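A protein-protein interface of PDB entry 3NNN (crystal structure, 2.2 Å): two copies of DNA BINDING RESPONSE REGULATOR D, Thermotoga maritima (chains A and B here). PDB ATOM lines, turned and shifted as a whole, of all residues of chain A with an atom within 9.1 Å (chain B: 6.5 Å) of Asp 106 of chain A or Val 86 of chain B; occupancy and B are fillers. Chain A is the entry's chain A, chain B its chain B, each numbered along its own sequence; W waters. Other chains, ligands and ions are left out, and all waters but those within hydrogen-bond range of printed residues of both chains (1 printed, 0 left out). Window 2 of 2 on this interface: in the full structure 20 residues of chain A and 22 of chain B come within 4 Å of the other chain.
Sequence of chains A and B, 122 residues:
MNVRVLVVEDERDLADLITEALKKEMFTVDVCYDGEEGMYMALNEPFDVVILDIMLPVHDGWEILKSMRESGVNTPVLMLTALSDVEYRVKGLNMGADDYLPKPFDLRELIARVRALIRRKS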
ATOM      1  N   LEU A  17      14.983   8.726  -3.833  1.00  0.00           N
ATOM      2  CA  LEU A  17      15.358  10.089  -4.165  1.00  0.00           C
ATOM      3  C   LEU A  17      14.786  10.413  -5.552  1.00  0.00           C
ATOM      4  O   LEU A  17      14.136  11.440  -5.765  1.00  0.00           O
ATOM      5  CB  LEU A  17      16.888  10.193  -4.170  1.00  0.00           C
ATOM      6  CG  LEU A  17      17.555  11.565  -4.271  1.00  0.00           C
ATOM      7  CD1 LEU A  17      17.331  12.143  -5.649  1.00  0.00           C
ATOM      8  CD2 LEU A  17      16.999  12.479  -3.195  1.00  0.00           C
ATOM      9  N   ILE A  18      15.035   9.517  -6.495  1.00  0.00           N
ATOM     10  CA  ILE A  18      14.557   9.683  -7.860  1.00  0.00           C
ATOM     11  C   ILE A  18      13.027   9.795  -7.892  1.00  0.00           C
ATOM     12  O   ILE A  18      12.471  10.698  -8.512  1.00  0.00           O
ATOM     13  CB  ILE A  18      15.036   8.492  -8.724  1.00  0.00           C
ATOM     14  CG1 ILE A  18      16.568   8.544  -8.812  1.00  0.00           C
ATOM     15  CG2 ILE A  18      14.382   8.525 -10.096  1.00  0.00           C
ATOM     16  CD1 ILE A  18      17.215   7.351  -9.487  1.00  0.00           C
ATOM     17  N   ALA A  21      11.575  13.110  -6.583  1.00  0.00           N
ATOM     18  CA  ALA A  21      11.795  14.162  -7.557  1.00  0.00           C
ATOM     19  C   ALA A  21      10.753  14.079  -8.671  1.00  0.00           C
ATOM     20  O   ALA A  21      10.196  15.095  -9.080  1.00  0.00           O
ATOM     21  CB  ALA A  21      13.197  14.052  -8.131  1.00  0.00           C
ATOM     22  N   LEU A  80      19.560   4.561 -16.362  1.00  0.00           N
ATOM     23  CA  LEU A  80      20.322   5.330 -15.370  1.00  0.00           C
ATOM     24  C   LEU A  80      21.186   4.286 -14.676  1.00  0.00           C
ATOM     25  O   LEU A  80      20.681   3.506 -13.869  1.00  0.00           O
ATOM     26  CB  LEU A  80      19.397   5.971 -14.330  1.00  0.00           C
ATOM     27  CG  LEU A  80      19.066   7.469 -14.383  1.00  0.00           C
ATOM     28  CD1 LEU A  80      18.273   7.835 -13.120  1.00  0.00           C
ATOM     29  CD2 LEU A  80      20.335   8.306 -14.456  1.00  0.00           C
ATOM     30  N   LEU A 101      21.608   7.830 -19.422  1.00  0.00           N
ATOM     31  CA  LEU A 101      22.219   8.828 -18.563  1.00  0.00           C
ATOM     32  C   LEU A 101      23.010   8.133 -17.464  1.00  0.00           C
ATOM     33  O   LEU A 101      22.451   7.526 -16.551  1.00  0.00           O
ATOM     34  CB  LEU A 101      21.134   9.724 -17.951  1.00  0.00           C
ATOM     35  CG  LEU A 101      21.578  10.939 -17.135  1.00  0.00           C
ATOM     36  CD1 LEU A 101      22.359  11.878 -18.029  1.00  0.00           C
ATOM     37  CD2 LEU A 101      20.361  11.668 -16.564  1.00  0.00           C
ATOM     38  N   PRO A 102      24.340   8.175 -17.566  1.00  0.00           N
ATOM     39  CA  PRO A 102      25.190   7.542 -16.560  1.00  0.00           C
ATOM     40  C   PRO A 102      25.150   8.240 -15.200  1.00  0.00           C
ATOM     41  O   PRO A 102      24.716   9.392 -15.076  1.00  0.00           O
ATOM     42  CB  PRO A 102      26.583   7.599 -17.200  1.00  0.00           C
ATOM     43  CG  PRO A 102      26.505   8.799 -18.086  1.00  0.00           C
ATOM     44  CD  PRO A 102      25.139   8.634 -18.715  1.00  0.00           C
ATOM     45  N   LYS A 103      25.585   7.510 -14.179  1.00  0.00           N
ATOM     46  CA  LYS A 103      25.664   8.030 -12.818  1.00  0.00           C
ATOM     47  C   LYS A 103      27.143   8.352 -12.664  1.00  0.00           C
ATOM     48  O   LYS A 103      27.980   7.716 -13.307  1.00  0.00           O
ATOM     49  CB  LYS A 103      25.282   6.957 -11.806  1.00  0.00           C
ATOM     50  CG  LYS A 103      23.925   6.322 -12.028  1.00  0.00           C
ATOM     51  CD  LYS A 103      23.665   5.267 -10.967  1.00  0.00           C
ATOM     52  CE  LYS A 103      22.348   4.553 -11.200  1.00  0.00           C
ATOM     53  NZ  LYS A 103      22.206   3.389 -10.291  1.00  0.00           N
ATOM     54  N   PRO A 104      27.481   9.352 -11.841  1.00  0.00           N
ATOM     55  CA  PRO A 104      26.511  10.154 -11.096  1.00  0.00           C
ATOM     56  C   PRO A 104      25.810  11.109 -12.052  1.00  0.00           C
ATOM     57  O   PRO A 104      26.409  11.600 -13.017  1.00  0.00           O
ATOM     58  CB  PRO A 104      27.379  10.869 -10.069  1.00  0.00           C
ATOM     59  CG  PRO A 104      28.653  11.094 -10.824  1.00  0.00           C
ATOM     60  CD  PRO A 104      28.860   9.769 -11.539  1.00  0.00           C
ATOM     61  N   PHE A 105      24.541  11.376 -11.789  1.00  0.00           N
ATOM     62  CA  PHE A 105      23.775  12.259 -12.655  1.00  0.00           C
ATOM     63  C   PHE A 105      23.291  13.504 -11.927  1.00  0.00           C
ATOM     64  O   PHE A 105      23.198  13.524 -10.701  1.00  0.00           O
ATOM     65  CB  PHE A 105      22.575  11.495 -13.216  1.00  0.00           C
ATOM     66  CG  PHE A 105      21.656  10.961 -12.152  1.00  0.00           C
ATOM     67  CD1 PHE A 105      20.753  11.802 -11.507  1.00  0.00           C
ATOM     68  CD2 PHE A 105      21.737   9.632 -11.747  1.00  0.00           C
ATOM     69  CE1 PHE A 105      19.948  11.332 -10.471  1.00  0.00           C
ATOM     70  CE2 PHE A 105      20.936   9.150 -10.710  1.00  0.00           C
ATOM     71  CZ  PHE A 105      20.042  10.003 -10.072  1.00  0.00           C
ATOM     72  N   ASP A 106      22.996  14.549 -12.689  1.00  0.00           N
ATOM     73  CA  ASP A 106      22.473  15.771 -12.107  1.00  0.00           C
ATOM     74  C   ASP A 106      20.954  15.619 -12.171  1.00  0.00           C
ATOM     75  O   ASP A 106      20.400  15.327 -13.229  1.00  0.00           O
ATOM     76  CB  ASP A 106      22.917  16.987 -12.911  1.00  0.00           C
ATOM     77  CG  ASP A 106      22.489  18.284 -12.267  1.00  0.00           C
ATOM     78  OD1 ASP A 106      21.279  18.450 -12.043  1.00  0.00           O
ATOM     79  OD2 ASP A 106      23.354  19.135 -11.977  1.00  0.00           O
ATOM     80  N   LEU A 107      20.290  15.816 -11.038  1.00  0.00           N
ATOM     81  CA  LEU A 107      18.841  15.659 -10.955  1.00  0.00           C
ATOM     82  C   LEU A 107      18.087  16.508 -11.964  1.00  0.00           C
ATOM     83  O   LEU A 107      17.053  16.095 -12.489  1.00  0.00           O
ATOM     84  CB  LEU A 107      18.362  15.997  -9.543  1.00  0.00           C
ATOM     85  CG  LEU A 107      16.990  15.452  -9.162  1.00  0.00           C
ATOM     86  CD1 LEU A 107      17.074  13.927  -9.024  1.00  0.00           C
ATOM     87  CD2 LEU A 107      16.518  16.080  -7.851  1.00  0.00           C
ATOM     88  N   ARG A 108      18.591  17.705 -12.229  1.00  0.00           N
ATOM     89  CA  ARG A 108      17.932  18.578 -13.187  1.00  0.00           C
ATOM     90  C   ARG A 108      17.999  17.970 -14.590  1.00  0.00           C
ATOM     91  O   ARG A 108      17.041  18.074 -15.357  1.00  0.00           O
ATOM     92  CB  ARG A 108      18.589  19.960 -13.175  1.00  0.00           C
ATOM     93  CG  ARG A 108      18.534  20.674 -11.817  1.00  0.00           C
ATOM     94  CD  ARG A 108      19.483  21.870 -11.811  1.00  0.00           C
ATOM     95  NE  ARG A 108      20.871  21.446 -11.999  1.00  0.00           N
ATOM     96  CZ  ARG A 108      21.893  22.266 -12.218  1.00  0.00           C
ATOM     97  NH1 ARG A 108      21.700  23.580 -12.283  1.00  0.00           N
ATOM     98  NH2 ARG A 108      23.115  21.767 -12.363  1.00  0.00           N
ATOM     99  N   GLU A 109      19.112  17.324 -14.927  1.00  0.00           N
ATOM    100  CA  GLU A 109      19.216  16.730 -16.253  1.00  0.00           C
ATOM    101  C   GLU A 109      18.303  15.518 -16.402  1.00  0.00           C
ATOM    102  O   GLU A 109      17.699  15.314 -17.450  1.00  0.00           O
ATOM    103  CB  GLU A 109      20.651  16.329 -16.582  1.00  0.00           C
ATOM    104  CG  GLU A 109      20.801  16.068 -18.076  1.00  0.00           C
ATOM    105  CD  GLU A 109      22.219  15.836 -18.515  1.00  0.00           C
ATOM    106  OE1 GLU A 109      22.430  15.647 -19.739  1.00  0.00           O
ATOM    107  OE2 GLU A 109      23.118  15.844 -17.644  1.00  0.00           O
ATOM    108  N   LEU A 110      18.214  14.714 -15.348  1.00  0.00           N
ATOM    109  CA  LEU A 110      17.360  13.541 -15.356  1.00  0.00           C
ATOM    110  C   LEU A 110      15.907  13.976 -15.633  1.00  0.00           C
ATOM    111  O   LEU A 110      15.275  13.486 -16.567  1.00  0.00           O
ATOM    112  CB  LEU A 110      17.452  12.830 -14.007  1.00  0.00           C
ATOM    113  CG  LEU A 110      17.145  11.327 -13.838  1.00  0.00           C
ATOM    114  CD1 LEU A 110      16.679  11.098 -12.415  1.00  0.00           C
ATOM    115  CD2 LEU A 110      16.098  10.816 -14.812  1.00  0.00           C
ATOM    116  N   ILE A 111      15.377  14.902 -14.836  1.00  0.00           N
ATOM    117  CA  ILE A 111      13.999  15.354 -15.039  1.00  0.00           C
ATOM    118  C   ILE A 111      13.795  15.936 -16.430  1.00  0.00           C
ATOM    119  O   ILE A 111      12.803  15.646 -17.096  1.00  0.00           O
ATOM    120  CB  ILE A 111      13.573  16.376 -13.940  1.00  0.00           C
ATOM    121  CG1 ILE A 111      13.100  15.608 -12.702  1.00  0.00           C
ATOM    122  CG2 ILE A 111      12.452  17.297 -14.433  1.00  0.00           C
ATOM    123  CD1 ILE A 111      14.206  14.952 -11.945  1.00  0.00           C
ATOM    124  N   ALA A 112      14.753  16.740 -16.877  1.00  0.00           N
ATOM    125  CA  ALA A 112      14.676  17.345 -18.199  1.00  0.00           C
ATOM    126  C   ALA A 112      14.606  16.262 -19.278  1.00  0.00           C
ATOM    127  O   ALA A 112      13.859  16.399 -20.248  1.00  0.00           O
ATOM    128  CB  ALA A 112      15.887  18.238 -18.423  1.00  0.00           C
ATOM    129  N   ARG A 113      15.375  15.185 -19.115  1.00  0.00           N
ATOM    130  CA  ARG A 113      15.369  14.105 -20.113  1.00  0.00           C
ATOM    131  C   ARG A 113      14.130  13.228 -20.048  1.00  0.00           C
ATOM    132  O   ARG A 113      13.676  12.704 -21.066  1.00  0.00           O
ATOM    133  CB  ARG A 113      16.636  13.243 -19.992  1.00  0.00           C
ATOM    134  CG  ARG A 113      17.880  13.955 -20.504  1.00  0.00           C
ATOM    135  CD  ARG A 113      19.170  13.134 -20.360  1.00  0.00           C
ATOM    136  NE  ARG A 113      20.336  13.892 -20.818  1.00  0.00           N
ATOM    137  CZ  ARG A 113      20.695  14.048 -22.093  1.00  0.00           C
ATOM    138  NH1 ARG A 113      19.993  13.487 -23.068  1.00  0.00           N
ATOM    139  NH2 ARG A 113      21.750  14.795 -22.398  1.00  0.00           N
ATOM    140  N   LEU B  83      28.767  23.798 -25.951  1.00  0.00           N
ATOM    141  CA  LEU B  83      28.187  24.356 -24.728  1.00  0.00           C
ATOM    142  C   LEU B  83      27.850  23.097 -23.933  1.00  0.00           C
ATOM    143  O   LEU B  83      26.729  22.584 -23.976  1.00  0.00           O
ATOM    144  CB  LEU B  83      26.915  25.150 -25.010  1.00  0.00           C
ATOM    145  CG  LEU B  83      27.100  26.358 -25.934  1.00  0.00           C
ATOM    146  CD1 LEU B  83      25.766  27.042 -26.132  1.00  0.00           C
ATOM    147  CD2 LEU B  83      28.103  27.334 -25.331  1.00  0.00           C
ATOM    148  N   SER B  84      28.843  22.611 -23.206  1.00  0.00           N
ATOM    149  CA  SER B  84      28.734  21.371 -22.449  1.00  0.00           C
ATOM    150  C   SER B  84      28.145  21.435 -21.047  1.00  0.00           C
ATOM    151  O   SER B  84      27.683  20.421 -20.526  1.00  0.00           O
ATOM    152  CB  SER B  84      30.121  20.757 -22.362  1.00  0.00           C
ATOM    153  OG  SER B  84      30.978  21.668 -21.703  1.00  0.00           O
ATOM    154  N   ASP B  85      28.190  22.606 -20.424  1.00  0.00           N
ATOM    155  CA  ASP B  85      27.664  22.773 -19.071  1.00  0.00           C
ATOM    156  C   ASP B  85      26.246  22.209 -18.950  1.00  0.00           C
ATOM    157  O   ASP B  85      25.383  22.481 -19.782  1.00  0.00           O
ATOM    158  CB  ASP B  85      27.672  24.258 -18.692  1.00  0.00           C
ATOM    159  CG  ASP B  85      27.185  24.512 -17.275  1.00  0.00           C
ATOM    160  OD1 ASP B  85      27.160  25.692 -16.866  1.00  0.00           O
ATOM    161  OD2 ASP B  85      26.825  23.546 -16.561  1.00  0.00           O
ATOM    162  N   VAL B  86      26.021  21.427 -17.901  1.00  0.00           N
ATOM    163  CA  VAL B  86      24.726  20.812 -17.669  1.00  0.00           C
ATOM    164  C   VAL B  86      23.580  21.818 -17.780  1.00  0.00           C
ATOM    165  O   VAL B  86      22.524  21.499 -18.335  1.00  0.00           O
ATOM    166  CB  VAL B  86      24.691  20.094 -16.285  1.00  0.00           C
ATOM    167  CG1 VAL B  86      24.911  21.105 -15.159  1.00  0.00           C
ATOM    168  CG2 VAL B  86      23.373  19.354 -16.095  1.00  0.00           C
ATOM    169  N   GLU B  87      23.773  23.040 -17.287  1.00  0.00           N
ATOM    170  CA  GLU B  87      22.686  24.012 -17.372  1.00  0.00           C
ATOM    171  C   GLU B  87      22.311  24.354 -18.813  1.00  0.00           C
ATOM    172  O   GLU B  87      21.163  24.703 -19.079  1.00  0.00           O
ATOM    173  CB  GLU B  87      23.009  25.269 -16.549  1.00  0.00           C
ATOM    174  CG  GLU B  87      23.101  24.957 -15.050  1.00  0.00           C
ATOM    175  CD  GLU B  87      23.026  26.179 -14.148  1.00  0.00           C
ATOM    176  OE1 GLU B  87      23.085  26.000 -12.903  1.00  0.00           O
ATOM    177  OE2 GLU B  87      22.905  27.315 -14.668  1.00  0.00           O
ATOM    178  N   TYR B  88      23.261  24.233 -19.741  1.00  0.00           N
ATOM    179  CA  TYR B  88      22.958  24.490 -21.149  1.00  0.00           C
ATOM    180  C   TYR B  88      22.165  23.282 -21.665  1.00  0.00           C
ATOM    181  O   TYR B  88      21.206  23.422 -22.430  1.00  0.00           O
ATOM    182  CB  TYR B  88      24.240  24.666 -21.967  1.00  0.00           C
ATOM    183  CG  TYR B  88      25.100  25.838 -21.530  1.00  0.00           C
ATOM    184  CD1 TYR B  88      24.531  27.090 -21.257  1.00  0.00           C
ATOM    185  CD2 TYR B  88      26.487  25.705 -21.417  1.00  0.00           C
ATOM    186  CE1 TYR B  88      25.328  28.182 -20.882  1.00  0.00           C
ATOM    187  CE2 TYR B  88      27.294  26.782 -21.050  1.00  0.00           C
ATOM    188  CZ  TYR B  88      26.713  28.015 -20.784  1.00  0.00           C
ATOM    189  OH  TYR B  88      27.515  29.073 -20.423  1.00  0.00           O
ATOM    190  N   ARG B  89      22.563  22.092 -21.228  1.00  0.00           N
ATOM    191  CA  ARG B  89      21.876  20.877 -21.634  1.00  0.00           C
ATOM    192  C   ARG B  89      20.409  20.935 -21.210  1.00  0.00           C
ATOM    193  O   ARG B  89      19.524  20.634 -21.999  1.00  0.00           O
ATOM    194  CB  ARG B  89      22.543  19.645 -21.007  1.00  0.00           C
ATOM    195  CG  ARG B  89      24.052  19.560 -21.220  1.00  0.00           C
ATOM    196  CD  ARG B  89      24.556  18.117 -21.219  1.00  0.00           C
ATOM    197  NE  ARG B  89      24.613  17.465 -19.907  1.00  0.00           N
ATOM    198  CZ  ARG B  89      25.685  17.446 -19.116  1.00  0.00           C
ATOM    199  NH1 ARG B  89      26.803  18.057 -19.486  1.00  0.00           N
ATOM    200  NH2 ARG B  89      25.663  16.764 -17.978  1.00  0.00           N
ATOM    201  N   VAL B  90      20.148  21.335 -19.971  1.00  0.00           N
ATOM    202  CA  VAL B  90      18.768  21.391 -19.478  1.00  0.00           C
ATOM    203  C   VAL B  90      17.949  22.413 -20.258  1.00  0.00           C
ATOM    204  O   VAL B  90      16.799  22.160 -20.619  1.00  0.00           O
ATOM    205  CB  VAL B  90      18.738  21.697 -17.967  1.00  0.00           C
ATOM    206  CG1 VAL B  90      17.307  21.902 -17.490  1.00  0.00           C
ATOM    207  CG2 VAL B  90      19.383  20.549 -17.216  1.00  0.00           C
ATOM    208  N   LYS B  91      18.558  23.555 -20.536  1.00  0.00           N
ATOM    209  CA  LYS B  91      17.895  24.599 -21.304  1.00  0.00           C
ATOM    210  C   LYS B  91      17.538  24.049 -22.685  1.00  0.00           C
ATOM    211  O   LYS B  91      16.434  24.268 -23.195  1.00  0.00           O
ATOM    212  CB  LYS B  91      18.820  25.812 -21.442  1.00  0.00           C
ATOM    213  CG  LYS B  91      18.372  26.809 -22.502  1.00  0.00           C
ATOM    214  CD  LYS B  91      19.288  28.016 -22.569  1.00  0.00           C
ATOM    215  CE  LYS B  91      18.956  28.893 -23.779  1.00  0.00           C
ATOM    216  NZ  LYS B  91      17.550  29.398 -23.758  1.00  0.00           N
HETATM  217  O   HOH W   1      25.045  23.861 -12.580  1.00  0.00           O
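The guanidinium group (NH1) of Arg 108 of chain A is in salt-bridge range of the side-chain carboxylate (OE1) of Glu 87 of chain B (2.9 Å).
The guanidinium group (NH2) of Arg 89 of chain B lies within salt-bridge range of the side-chain carboxylate (OE2) of Glu 109 of chain A (2.7 Å).
The side-chain carboxylate (OD2) of Asp 106 of chain A is in salt-bridge range of the guanidinium group (NH2) of Arg 108 of chain A, at 2.7 Å.
The side-chain carboxylate (OE1) of Glu 109 of chain A is in salt-bridge range of the guanidinium group (NH2) of Arg 113 of chain A.
NH1 of Arg 89 of chain B sits at hydrogen-bond distance from O of Ser 84 of chain B, 2.7 Å away.
The side-chain carboxylate (OD2) of Asp 85 of chain B sits close to the backbone NH (N) of Glu 87 of chain B (3.2 Å).
Among the printed residues, pairs that only touch across the chains: Arg 108 of chain A with Val 86 of chain B, Glu 109 of chain A with Val 86 of chain B, Arg 108 of chain A with Val 90 of chain B, Glu 109 of chain A with Val 90 of chain B and Asp 106 of chain A with Val 86 of chain B.
Of the printed residues of chain B, Asp 106 of chain A touches Val 86 (3.99 Å).
Of the printed residues of chain B, Arg 108 of chain A touches Val 86 (3.4 Å), Glu 87 (2.9 Å) and Val 90 (3.9 Å).
Ala 112 of chain A touches none of the printed residues of chain B.
Arg 113 of chain A touches none of the printed residues of chain B.
No residue of chain A comes within 4 Å of Asp 85 of chain B.
Of the printed residues of chain A, Val 86 of chain B touches Asp 106, Arg 108 and Glu 109.
Printed residues of chain A within 4 Å of Glu 87 of chain B: Arg 108.
Arg 89 of chain B touches one residue of chain A.
Printed residues of chain A within 4 Å of Val 90 of chain B: Arg 108 (3.9 Å) and Glu 109 (3.9 Å).
The nearest printed residue of chain B that does not touch Arg 108 of chain A is Asp 85 of chain B (5.9 Å).
Among the printed residues, Asp or Glu carboxylates within 4 Å of a Lys or Arg side-chain nitrogen of the other chain: Arg 108 of chain A with Glu 87 of chain B (2.9 Å) and Glu 109 of chain A with Arg 89 of chain B (2.7 Å).
No position is printed for both chains.
Of the 7 pairs that touch across the chains among the printed residues, none has its exchanged pair printed and touching as well.
Water W1 bridges NH2 of Arg 108 of chain A (2.9 Å) and OE1 of Glu 87 of chain B (2.9 Å).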
